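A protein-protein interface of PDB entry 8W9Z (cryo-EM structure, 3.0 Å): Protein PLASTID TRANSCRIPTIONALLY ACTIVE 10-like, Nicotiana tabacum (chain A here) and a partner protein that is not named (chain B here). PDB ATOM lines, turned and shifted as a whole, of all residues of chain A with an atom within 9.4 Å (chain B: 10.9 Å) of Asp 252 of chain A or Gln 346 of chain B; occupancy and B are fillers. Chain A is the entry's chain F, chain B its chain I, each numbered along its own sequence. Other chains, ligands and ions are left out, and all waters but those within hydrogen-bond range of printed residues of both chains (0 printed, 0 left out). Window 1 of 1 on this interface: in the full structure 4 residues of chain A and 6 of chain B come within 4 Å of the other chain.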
ATOM      1  N   SER A 246     -20.404   0.513  -8.412  1.00  0.00           N
ATOM      2  CA  SER A 246     -20.654  -0.732  -9.130  1.00  0.00           C
ATOM      3  C   SER A 246     -20.673  -0.505 -10.635  1.00  0.00           C
ATOM      4  O   SER A 246     -20.138  -1.315 -11.399  1.00  0.00           O
ATOM      5  CB  SER A 246     -21.972  -1.351  -8.665  1.00  0.00           C
ATOM      6  OG  SER A 246     -22.253  -2.540  -9.382  1.00  0.00           O
ATOM      7  N   TYR A 247     -21.287   0.594 -11.079  1.00  0.00           N
ATOM      8  CA  TYR A 247     -21.298   0.897 -12.508  1.00  0.00           C
ATOM      9  C   TYR A 247     -19.914   1.278 -13.017  1.00  0.00           C
ATOM     10  O   TYR A 247     -19.597   1.030 -14.185  1.00  0.00           O
ATOM     11  CB  TYR A 247     -22.295   2.016 -12.806  1.00  0.00           C
ATOM     12  CG  TYR A 247     -23.694   1.530 -13.101  1.00  0.00           C
ATOM     13  CD1 TYR A 247     -24.048   1.113 -14.377  1.00  0.00           C
ATOM     14  CD2 TYR A 247     -24.663   1.492 -12.109  1.00  0.00           C
ATOM     15  CE1 TYR A 247     -25.324   0.669 -14.655  1.00  0.00           C
ATOM     16  CE2 TYR A 247     -25.943   1.050 -12.378  1.00  0.00           C
ATOM     17  CZ  TYR A 247     -26.268   0.640 -13.651  1.00  0.00           C
ATOM     18  OH  TYR A 247     -27.542   0.198 -13.925  1.00  0.00           O
ATOM     19  N   LYS A 248     -19.081   1.878 -12.166  1.00  0.00           N
ATOM     20  CA  LYS A 248     -17.774   2.341 -12.618  1.00  0.00           C
ATOM     21  C   LYS A 248     -16.766   1.200 -12.705  1.00  0.00           C
ATOM     22  O   LYS A 248     -16.087   1.042 -13.726  1.00  0.00           O
ATOM     23  CB  LYS A 248     -17.256   3.439 -11.688  1.00  0.00           C
ATOM     24  CG  LYS A 248     -15.914   4.017 -12.105  1.00  0.00           C
ATOM     25  CD  LYS A 248     -15.478   5.136 -11.174  1.00  0.00           C
ATOM     26  CE  LYS A 248     -14.147   5.727 -11.610  1.00  0.00           C
ATOM     27  NZ  LYS A 248     -13.709   6.831 -10.712  1.00  0.00           N
ATOM     28  N   TYR A 249     -16.652   0.394 -11.649  1.00  0.00           N
ATOM     29  CA  TYR A 249     -15.609  -0.623 -11.597  1.00  0.00           C
ATOM     30  C   TYR A 249     -16.011  -1.934 -12.259  1.00  0.00           C
ATOM     31  O   TYR A 249     -15.147  -2.628 -12.805  1.00  0.00           O
ATOM     32  CB  TYR A 249     -15.199  -0.885 -10.144  1.00  0.00           C
ATOM     33  CG  TYR A 249     -14.642   0.336  -9.448  1.00  0.00           C
ATOM     34  CD1 TYR A 249     -13.333   0.744  -9.661  1.00  0.00           C
ATOM     35  CD2 TYR A 249     -15.427   1.082  -8.583  1.00  0.00           C
ATOM     36  CE1 TYR A 249     -12.823   1.862  -9.030  1.00  0.00           C
ATOM     37  CE2 TYR A 249     -14.929   2.202  -7.949  1.00  0.00           C
ATOM     38  CZ  TYR A 249     -13.627   2.587  -8.175  1.00  0.00           C
ATOM     39  OH  TYR A 249     -13.133   3.703  -7.541  1.00  0.00           O
ATOM     40  N   ASP A 250     -17.292  -2.289 -12.227  1.00  0.00           N
ATOM     41  CA  ASP A 250     -17.778  -3.517 -12.842  1.00  0.00           C
ATOM     42  C   ASP A 250     -18.491  -3.183 -14.145  1.00  0.00           C
ATOM     43  O   ASP A 250     -19.393  -2.339 -14.166  1.00  0.00           O
ATOM     44  CB  ASP A 250     -18.719  -4.266 -11.897  1.00  0.00           C
ATOM     45  CG  ASP A 250     -18.036  -4.689 -10.611  1.00  0.00           C
ATOM     46  OD1 ASP A 250     -16.807  -4.906 -10.634  1.00  0.00           O
ATOM     47  OD2 ASP A 250     -18.729  -4.806  -9.578  1.00  0.00           O
ATOM     48  N   GLN A 251     -18.087  -3.847 -15.227  1.00  0.00           N
ATOM     49  CA  GLN A 251     -18.627  -3.558 -16.552  1.00  0.00           C
ATOM     50  C   GLN A 251     -19.857  -4.408 -16.861  1.00  0.00           C
ATOM     51  O   GLN A 251     -20.945  -3.873 -17.097  1.00  0.00           O
ATOM     52  CB  GLN A 251     -17.548  -3.773 -17.617  1.00  0.00           C
ATOM     53  CG  GLN A 251     -18.054  -3.637 -19.041  1.00  0.00           C
ATOM     54  CD  GLN A 251     -16.955  -3.803 -20.071  1.00  0.00           C
ATOM     55  OE1 GLN A 251     -17.198  -3.714 -21.273  1.00  0.00           O
ATOM     56  NE2 GLN A 251     -15.737  -4.046 -19.602  1.00  0.00           N
ATOM     57  N   ASP A 252     -19.700  -5.727 -16.860  1.00  0.00           N
ATOM     58  CA  ASP A 252     -20.782  -6.646 -17.177  1.00  0.00           C
ATOM     59  C   ASP A 252     -21.237  -7.368 -15.916  1.00  0.00           C
ATOM     60  O   ASP A 252     -20.420  -7.715 -15.057  1.00  0.00           O
ATOM     61  CB  ASP A 252     -20.349  -7.666 -18.234  1.00  0.00           C
ATOM     62  CG  ASP A 252     -20.056  -7.024 -19.574  1.00  0.00           C
ATOM     63  OD1 ASP A 252     -20.673  -5.984 -19.885  1.00  0.00           O
ATOM     64  OD2 ASP A 252     -19.209  -7.559 -20.320  1.00  0.00           O
ATOM     65  N   TYR A 253     -22.542  -7.592 -15.813  1.00  0.00           N
ATOM     66  CA  TYR A 253     -23.092  -8.283 -14.658  1.00  0.00           C
ATOM     67  C   TYR A 253     -22.756  -9.767 -14.715  1.00  0.00           C
ATOM     68  O   TYR A 253     -22.708 -10.373 -15.789  1.00  0.00           O
ATOM     69  CB  TYR A 253     -24.606  -8.088 -14.590  1.00  0.00           C
ATOM     70  CG  TYR A 253     -25.277  -8.871 -13.485  1.00  0.00           C
ATOM     71  CD1 TYR A 253     -25.301  -8.390 -12.184  1.00  0.00           C
ATOM     72  CD2 TYR A 253     -25.891 -10.089 -13.744  1.00  0.00           C
ATOM     73  CE1 TYR A 253     -25.913  -9.102 -11.173  1.00  0.00           C
ATOM     74  CE2 TYR A 253     -26.504 -10.806 -12.739  1.00  0.00           C
ATOM     75  CZ  TYR A 253     -26.513 -10.309 -11.457  1.00  0.00           C
ATOM     76  OH  TYR A 253     -27.125 -11.021 -10.452  1.00  0.00           O
ATOM     77  N   TYR A 254     -22.523 -10.350 -13.543  1.00  0.00           N
ATOM     78  CA  TYR A 254     -22.219 -11.764 -13.397  1.00  0.00           C
ATOM     79  C   TYR A 254     -22.731 -12.202 -12.037  1.00  0.00           C
ATOM     80  O   TYR A 254     -22.765 -11.388 -11.106  1.00  0.00           O
ATOM     81  CB  TYR A 254     -20.711 -12.028 -13.517  1.00  0.00           C
ATOM     82  CG  TYR A 254     -20.341 -13.487 -13.643  1.00  0.00           C
ATOM     83  CD1 TYR A 254     -20.433 -14.141 -14.863  1.00  0.00           C
ATOM     84  CD2 TYR A 254     -19.895 -14.210 -12.545  1.00  0.00           C
ATOM     85  CE1 TYR A 254     -20.096 -15.471 -14.986  1.00  0.00           C
ATOM     86  CE2 TYR A 254     -19.556 -15.543 -12.661  1.00  0.00           C
ATOM     87  CZ  TYR A 254     -19.659 -16.167 -13.884  1.00  0.00           C
ATOM     88  OH  TYR A 254     -19.322 -17.494 -14.006  1.00  0.00           O
ATOM     89  N   PRO A 255     -23.165 -13.462 -11.893  1.00  0.00           N
ATOM     90  CA  PRO A 255     -23.590 -13.942 -10.571  1.00  0.00           C
ATOM     91  C   PRO A 255     -22.530 -13.711  -9.507  1.00  0.00           C
ATOM     92  O   PRO A 255     -21.449 -14.307  -9.548  1.00  0.00           O
ATOM     93  CB  PRO A 255     -23.840 -15.435 -10.811  1.00  0.00           C
ATOM     94  CG  PRO A 255     -24.254 -15.502 -12.235  1.00  0.00           C
ATOM     95  CD  PRO A 255     -23.453 -14.445 -12.952  1.00  0.00           C
ATOM     96  N   GLY A 256     -22.838 -12.841  -8.550  1.00  0.00           N
ATOM     97  CA  GLY A 256     -21.901 -12.428  -7.522  1.00  0.00           C
ATOM     98  C   GLY A 256     -21.641 -10.937  -7.484  1.00  0.00           C
ATOM     99  O   GLY A 256     -21.094 -10.441  -6.489  1.00  0.00           O
ATOM    100  N   ARG A 257     -22.012 -10.205  -8.531  1.00  0.00           N
ATOM    101  CA  ARG A 257     -21.819  -8.766  -8.575  1.00  0.00           C
ATOM    102  C   ARG A 257     -23.064  -8.054  -8.051  1.00  0.00           C
ATOM    103  O   ARG A 257     -24.069  -8.675  -7.697  1.00  0.00           O
ATOM    104  CB  ARG A 257     -21.485  -8.314  -9.997  1.00  0.00           C
ATOM    105  CG  ARG A 257     -20.174  -8.859 -10.548  1.00  0.00           C
ATOM    106  CD  ARG A 257     -18.962  -8.225  -9.880  1.00  0.00           C
ATOM    107  NE  ARG A 257     -18.603  -8.883  -8.627  1.00  0.00           N
ATOM    108  CZ  ARG A 257     -17.611  -8.492  -7.835  1.00  0.00           C
ATOM    109  NH1 ARG A 257     -16.872  -7.442  -8.162  1.00  0.00           N
ATOM    110  NH2 ARG A 257     -17.356  -9.150  -6.713  1.00  0.00           N
ATOM    111  N   ARG A 258     -22.996  -6.726  -7.998  1.00  0.00           N
ATOM    112  CA  ARG A 258     -24.093  -5.942  -7.448  1.00  0.00           C
ATOM    113  C   ARG A 258     -25.248  -5.872  -8.437  1.00  0.00           C
ATOM    114  O   ARG A 258     -25.056  -5.542  -9.612  1.00  0.00           O
ATOM    115  CB  ARG A 258     -23.611  -4.537  -7.094  1.00  0.00           C
ATOM    116  CG  ARG A 258     -24.700  -3.637  -6.541  1.00  0.00           C
ATOM    117  CD  ARG A 258     -24.128  -2.389  -5.897  1.00  0.00           C
ATOM    118  NE  ARG A 258     -25.169  -1.591  -5.256  1.00  0.00           N
ATOM    119  CZ  ARG A 258     -25.593  -1.781  -4.012  1.00  0.00           C
ATOM    120  NH1 ARG A 258     -25.067  -2.744  -3.270  1.00  0.00           N
ATOM    121  NH2 ARG A 258     -26.545  -1.008  -3.510  1.00  0.00           N
ATOM    122  N   ARG A 260     -27.991  -4.283 -10.378  1.00  0.00           N
ATOM    123  CA  ARG A 260     -28.147  -2.901 -10.803  1.00  0.00           C
ATOM    124  C   ARG A 260     -29.140  -2.829 -11.953  1.00  0.00           C
ATOM    125  O   ARG A 260     -29.454  -3.833 -12.597  1.00  0.00           O
ATOM    126  CB  ARG A 260     -26.802  -2.297 -11.221  1.00  0.00           C
ATOM    127  CG  ARG A 260     -26.075  -3.113 -12.276  1.00  0.00           C
ATOM    128  CD  ARG A 260     -24.647  -2.636 -12.459  1.00  0.00           C
ATOM    129  NE  ARG A 260     -23.950  -3.401 -13.488  1.00  0.00           N
ATOM    130  CZ  ARG A 260     -22.667  -3.245 -13.793  1.00  0.00           C
ATOM    131  NH1 ARG A 260     -21.933  -2.352 -13.145  1.00  0.00           N
ATOM    132  NH2 ARG A 260     -22.117  -3.983 -14.746  1.00  0.00           N
ATOM    133  N   ASP A 263     -32.686  -5.016 -12.350  1.00  0.00           N
ATOM    134  CA  ASP A 263     -32.633  -6.113 -11.394  1.00  0.00           C
ATOM    135  C   ASP A 263     -32.605  -5.646  -9.944  1.00  0.00           C
ATOM    136  O   ASP A 263     -32.616  -6.490  -9.042  1.00  0.00           O
ATOM    137  CB  ASP A 263     -31.409  -6.989 -11.670  1.00  0.00           C
ATOM    138  CG  ASP A 263     -31.413  -7.570 -13.069  1.00  0.00           C
ATOM    139  OD1 ASP A 263     -32.513  -7.809 -13.611  1.00  0.00           O
ATOM    140  OD2 ASP A 263     -30.318  -7.790 -13.627  1.00  0.00           O
ATOM    141  N   ARG A 339     -14.277 -12.022  -6.261  1.00  0.00           N
ATOM    142  CA  ARG A 339     -15.379 -12.127  -7.211  1.00  0.00           C
ATOM    143  C   ARG A 339     -16.691 -12.425  -6.501  1.00  0.00           C
ATOM    144  O   ARG A 339     -17.709 -11.769  -6.751  1.00  0.00           O
ATOM    145  CB  ARG A 339     -15.073 -13.207  -8.250  1.00  0.00           C
ATOM    146  CG  ARG A 339     -13.836 -12.941  -9.083  1.00  0.00           C
ATOM    147  CD  ARG A 339     -13.677 -13.986 -10.170  1.00  0.00           C
ATOM    148  NE  ARG A 339     -14.823 -14.007 -11.073  1.00  0.00           N
ATOM    149  CZ  ARG A 339     -14.964 -14.859 -12.082  1.00  0.00           C
ATOM    150  NH1 ARG A 339     -14.029 -15.766 -12.322  1.00  0.00           N
ATOM    151  NH2 ARG A 339     -16.040 -14.804 -12.852  1.00  0.00           N
ATOM    152  N   PHE A 365      -9.806 -10.666  -8.243  1.00  0.00           N
ATOM    153  CA  PHE A 365      -9.759  -9.891  -9.476  1.00  0.00           C
ATOM    154  C   PHE A 365      -8.344  -9.375  -9.697  1.00  0.00           C
ATOM    155  O   PHE A 365      -7.774  -8.719  -8.819  1.00  0.00           O
ATOM    156  CB  PHE A 365     -10.735  -8.714  -9.428  1.00  0.00           C
ATOM    157  CG  PHE A 365     -12.137  -9.061  -9.839  1.00  0.00           C
ATOM    158  CD1 PHE A 365     -12.440  -9.306 -11.166  1.00  0.00           C
ATOM    159  CD2 PHE A 365     -13.155  -9.113  -8.905  1.00  0.00           C
ATOM    160  CE1 PHE A 365     -13.728  -9.613 -11.549  1.00  0.00           C
ATOM    161  CE2 PHE A 365     -14.445  -9.420  -9.283  1.00  0.00           C
ATOM    162  CZ  PHE A 365     -14.732  -9.672 -10.606  1.00  0.00           C
ATOM    163  N   HIS A 366      -7.783  -9.670 -10.867  1.00  0.00           N
ATOM    164  CA  HIS A 366      -6.489  -9.132 -11.281  1.00  0.00           C
ATOM    165  C   HIS A 366      -6.773  -7.925 -12.170  1.00  0.00           C
ATOM    166  O   HIS A 366      -6.834  -8.031 -13.395  1.00  0.00           O
ATOM    167  CB  HIS A 366      -5.660 -10.187 -12.003  1.00  0.00           C
ATOM    168  CG  HIS A 366      -5.244 -11.329 -11.131  1.00  0.00           C
ATOM    169  ND1 HIS A 366      -3.948 -11.500 -10.697  1.00  0.00           N
ATOM    170  CD2 HIS A 366      -5.952 -12.360 -10.611  1.00  0.00           C
ATOM    171  CE1 HIS A 366      -3.875 -12.584  -9.947  1.00  0.00           C
ATOM    172  NE2 HIS A 366      -5.078 -13.125  -9.880  1.00  0.00           N
ATOM    173  N   ARG A 367      -6.946  -6.767 -11.540  1.00  0.00           N
ATOM    174  CA  ARG A 367      -7.385  -5.569 -12.241  1.00  0.00           C
ATOM    175  C   ARG A 367      -6.186  -4.860 -12.866  1.00  0.00           C
ATOM    176  O   ARG A 367      -5.073  -5.391 -12.922  1.00  0.00           O
ATOM    177  CB  ARG A 367      -8.152  -4.657 -11.288  1.00  0.00           C
ATOM    178  CG  ARG A 367      -8.982  -5.408 -10.265  1.00  0.00           C
ATOM    179  CD  ARG A 367      -9.844  -4.464  -9.452  1.00  0.00           C
ATOM    180  NE  ARG A 367     -11.029  -4.038 -10.189  1.00  0.00           N
ATOM    181  CZ  ARG A 367     -12.224  -4.607 -10.070  1.00  0.00           C
ATOM    182  NH1 ARG A 367     -13.248  -4.156 -10.778  1.00  0.00           N
ATOM    183  NH2 ARG A 367     -12.395  -5.623  -9.236  1.00  0.00           N
ATOM    184  N   ASP A 368      -6.409  -3.639 -13.354  1.00  0.00           N
ATOM    185  CA  ASP A 368      -5.353  -2.839 -13.957  1.00  0.00           C
ATOM    186  C   ASP A 368      -4.735  -1.837 -12.994  1.00  0.00           C
ATOM    187  O   ASP A 368      -3.629  -1.353 -13.257  1.00  0.00           O
ATOM    188  CB  ASP A 368      -5.890  -2.087 -15.181  1.00  0.00           C
ATOM    189  CG  ASP A 368      -6.463  -3.017 -16.230  1.00  0.00           C
ATOM    190  OD1 ASP A 368      -5.961  -4.153 -16.354  1.00  0.00           O
ATOM    191  OD2 ASP A 368      -7.415  -2.613 -16.929  1.00  0.00           O
ATOM    192  N   ASN B 342     -15.852  -0.619 -29.445  1.00  0.00           N
ATOM    193  CA  ASN B 342     -14.850  -1.253 -28.594  1.00  0.00           C
ATOM    194  C   ASN B 342     -15.484  -1.696 -27.282  1.00  0.00           C
ATOM    195  O   ASN B 342     -14.963  -1.442 -26.193  1.00  0.00           O
ATOM    196  CB  ASN B 342     -13.678  -0.314 -28.331  1.00  0.00           C
ATOM    197  CG  ASN B 342     -13.036   0.193 -29.603  1.00  0.00           C
ATOM    198  OD1 ASN B 342     -12.921  -0.537 -30.589  1.00  0.00           O
ATOM    199  ND2 ASN B 342     -12.612   1.450 -29.593  1.00  0.00           N
ATOM    200  N   TYR B 343     -16.638  -2.359 -27.376  1.00  0.00           N
ATOM    201  CA  TYR B 343     -17.382  -2.740 -26.180  1.00  0.00           C
ATOM    202  C   TYR B 343     -16.602  -3.742 -25.335  1.00  0.00           C
ATOM    203  O   TYR B 343     -16.558  -3.632 -24.104  1.00  0.00           O
ATOM    204  CB  TYR B 343     -18.748  -3.307 -26.574  1.00  0.00           C
ATOM    205  CG  TYR B 343     -19.528  -3.873 -25.412  1.00  0.00           C
ATOM    206  CD1 TYR B 343     -20.095  -3.037 -24.461  1.00  0.00           C
ATOM    207  CD2 TYR B 343     -19.704  -5.243 -25.270  1.00  0.00           C
ATOM    208  CE1 TYR B 343     -20.809  -3.549 -23.398  1.00  0.00           C
ATOM    209  CE2 TYR B 343     -20.420  -5.764 -24.207  1.00  0.00           C
ATOM    210  CZ  TYR B 343     -20.970  -4.911 -23.276  1.00  0.00           C
ATOM    211  OH  TYR B 343     -21.684  -5.414 -22.213  1.00  0.00           O
ATOM    212  N   ARG B 344     -15.980  -4.731 -25.985  1.00  0.00           N
ATOM    213  CA  ARG B 344     -15.138  -5.726 -25.332  1.00  0.00           C
ATOM    214  C   ARG B 344     -15.909  -6.507 -24.272  1.00  0.00           C
ATOM    215  O   ARG B 344     -15.731  -6.263 -23.071  1.00  0.00           O
ATOM    216  CB  ARG B 344     -13.907  -5.067 -24.706  1.00  0.00           C
ATOM    217  N   PRO B 345     -16.784  -7.430 -24.669  1.00  0.00           N
ATOM    218  CA  PRO B 345     -17.416  -8.307 -23.680  1.00  0.00           C
ATOM    219  C   PRO B 345     -16.370  -9.151 -22.963  1.00  0.00           C
ATOM    220  O   PRO B 345     -15.408  -9.629 -23.567  1.00  0.00           O
ATOM    221  CB  PRO B 345     -18.360  -9.172 -24.524  1.00  0.00           C
ATOM    222  N   GLN B 346     -16.560  -9.325 -21.657  1.00  0.00           N
ATOM    223  CA  GLN B 346     -15.563  -9.990 -20.827  1.00  0.00           C
ATOM    224  C   GLN B 346     -15.977 -11.382 -20.371  1.00  0.00           C
ATOM    225  O   GLN B 346     -15.126 -12.272 -20.282  1.00  0.00           O
ATOM    226  CB  GLN B 346     -15.233  -9.128 -19.603  1.00  0.00           C
ATOM    227  CG  GLN B 346     -16.441  -8.651 -18.823  1.00  0.00           C
ATOM    228  CD  GLN B 346     -16.056  -7.832 -17.607  1.00  0.00           C
ATOM    229  OE1 GLN B 346     -14.878  -7.707 -17.278  1.00  0.00           O
ATOM    230  NE2 GLN B 346     -17.052  -7.267 -16.935  1.00  0.00           N
ATOM    231  N   TYR B 347     -17.259 -11.604 -20.076  1.00  0.00           N
ATOM    232  CA  TYR B 347     -17.694 -12.904 -19.579  1.00  0.00           C
ATOM    233  C   TYR B 347     -18.156 -13.826 -20.706  1.00  0.00           C
ATOM    234  O   TYR B 347     -17.607 -14.918 -20.886  1.00  0.00           O
ATOM    235  CB  TYR B 347     -18.807 -12.723 -18.540  1.00  0.00           C
ATOM    236  CG  TYR B 347     -18.351 -12.029 -17.278  1.00  0.00           C
ATOM    237  CD1 TYR B 347     -17.585 -12.697 -16.336  1.00  0.00           C
ATOM    238  CD2 TYR B 347     -18.691 -10.706 -17.028  1.00  0.00           C
ATOM    239  CE1 TYR B 347     -17.165 -12.069 -15.183  1.00  0.00           C
ATOM    240  CE2 TYR B 347     -18.274 -10.069 -15.875  1.00  0.00           C
ATOM    241  CZ  TYR B 347     -17.513 -10.756 -14.958  1.00  0.00           C
ATOM    242  OH  TYR B 347     -17.096 -10.129 -13.807  1.00  0.00           O
ATOM    243  N   PHE B 348     -19.159 -13.401 -21.472  1.00  0.00           N
ATOM    244  CA  PHE B 348     -19.734 -14.236 -22.517  1.00  0.00           C
ATOM    245  C   PHE B 348     -19.962 -13.404 -23.771  1.00  0.00           C
ATOM    246  O   PHE B 348     -19.752 -12.189 -23.790  1.00  0.00           O
ATOM    247  CB  PHE B 348     -21.055 -14.873 -22.070  1.00  0.00           C
ATOM    248  CG  PHE B 348     -21.014 -15.456 -20.689  1.00  0.00           C
ATOM    249  CD1 PHE B 348     -20.249 -16.578 -20.419  1.00  0.00           C
ATOM    250  CD2 PHE B 348     -21.749 -14.891 -19.663  1.00  0.00           C
ATOM    251  CE1 PHE B 348     -20.212 -17.118 -19.149  1.00  0.00           C
ATOM    252  CE2 PHE B 348     -21.718 -15.427 -18.391  1.00  0.00           C
ATOM    253  CZ  PHE B 348     -20.949 -16.543 -18.134  1.00  0.00           C
ATOM    254  N   ALA B 349     -20.397 -14.085 -24.829  1.00  0.00           N
ATOM    255  CA  ALA B 349     -20.821 -13.448 -26.070  1.00  0.00           C
ATOM    256  C   ALA B 349     -22.343 -13.507 -26.132  1.00  0.00           C
ATOM    257  O   ALA B 349     -22.924 -14.590 -26.268  1.00  0.00           O
ATOM    258  CB  ALA B 349     -20.191 -14.130 -27.280  1.00  0.00           C
ATOM    259  N   GLU B 350     -22.989 -12.345 -26.030  1.00  0.00           N
ATOM    260  CA  GLU B 350     -24.446 -12.312 -25.946  1.00  0.00           C
ATOM    261  C   GLU B 350     -25.088 -12.583 -27.301  1.00  0.00           C
ATOM    262  O   GLU B 350     -25.982 -13.429 -27.418  1.00  0.00           O
ATOM    263  CB  GLU B 350     -24.908 -10.965 -25.390  1.00  0.00           C
ATOM    264  N   ASN B 351     -24.646 -11.871 -28.340  1.00  0.00           N
ATOM    265  CA  ASN B 351     -25.270 -11.981 -29.654  1.00  0.00           C
ATOM    266  C   ASN B 351     -24.980 -13.304 -30.348  1.00  0.00           C
ATOM    267  O   ASN B 351     -25.518 -13.539 -31.435  1.00  0.00           O
ATOM    268  CB  ASN B 351     -24.816 -10.824 -30.546  1.00  0.00           C
ATOM    269  N   GLN B 354     -20.524 -12.581 -31.760  1.00  0.00           N
ATOM    270  CA  GLN B 354     -19.396 -11.746 -31.375  1.00  0.00           C
ATOM    271  C   GLN B 354     -18.182 -12.558 -30.949  1.00  0.00           C
ATOM    272  O   GLN B 354     -17.144 -11.970 -30.625  1.00  0.00           O
ATOM    273  CB  GLN B 354     -19.804 -10.798 -30.242  1.00  0.00           C
ATOM    274  N   THR B 355     -18.284 -13.887 -30.941  1.00  0.00           N
ATOM    275  CA  THR B 355     -17.152 -14.730 -30.577  1.00  0.00           C
ATOM    276  C   THR B 355     -16.110 -14.820 -31.681  1.00  0.00           C
ATOM    277  O   THR B 355     -14.948 -15.125 -31.393  1.00  0.00           O
ATOM    278  CB  THR B 355     -17.634 -16.137 -30.216  1.00  0.00           C
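Asp 252 of chain A touches just these residues of chain B: Tyr 343 (2.6 Å), Pro 345 (3.9 Å), Gln 346 (3.1 Å) and Tyr 347 (3.3 Å). Printed residues of chain A within 4 Å of Gln 346 of chain B: Gln 251 and Asp 252. Gln 251 of chain A touches three residues of chain B. Of chain A, only Asp 252 comes within 4 Å of Pro 345 of chain B. Printed residues of chain A within 4 Å of Phe 348 of chain B: Tyr 254. Printed residues of chain A within 4 Å of Arg 344 of chain B: Gln 251 (3.4 Å). Printed residues of chain B within 4 Å of Arg 339 of chain A: Tyr 347 (3.8 Å). Printed residues of chain B within 4 Å of Tyr 254 of chain A: Tyr 347 (3.5 Å) and Phe 348 (3.4 Å). Gly 256 of chain A touches none of the printed residues of chain B. Arg 258 of chain A touches none of the printed residues of chain B. The nearest residue of chain A that does not touch Gln 346 of chain B is Asp 250 of chain A (5.2 Å).
Printed residues of chain A that touch a printed residue of chain B: Gln 251, Asp 252, Tyr 254 and Arg 339. Of the 12 printed residues of chain B, 6 touch a printed residue of chain A. Among the printed residues, no Asp or Glu carboxylate lies within 4 Å of a Lys or Arg side-chain nitrogen of the other chain.
Among the printed residues, pairs that only touch across the chains: Gln 251 of chain A with Gln 346 of chain B (3.6 Å), Asp 252 of chain A with Pro 345 of chain B (3.9 Å), Asp 252 of chain A with Tyr 347 of chain B (3.3 Å), Tyr 254 of chain A with Tyr 347 of chain B (3.5 Å), Tyr 254 of chain A with Phe 348 of chain B (3.4 Å) and Arg 339 of chain A with Tyr 347 of chain B (3.8 Å).
O of Arg 339 of chain A lies within hydrogen-bond range of NH2 of Arg 257 of chain A (2.6 Å). The backbone carbonyl oxygen (O) of Gln 251 of chain A lies within hydrogen-bond range of the guanidinium group (NH2) of Arg 260 of chain A, at 2.6 Å.
The side-chain amide oxygen (OE1) of Gln 251 of chain A sits close to the backbone carbonyl oxygen (O) of Tyr 343 of chain B (2.9 Å). OH of Tyr 343 of chain B sits at hydrogen-bond distance from OD1 of Asp 252 of chain A (2.6 Å). The backbone NH of Asp 252 of chain A lies close to the side-chain amide nitrogen of Gln 346 of chain B (3.1 Å). O of Arg 344 of chain B sits close to OE1 of Gln 251 of chain A.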
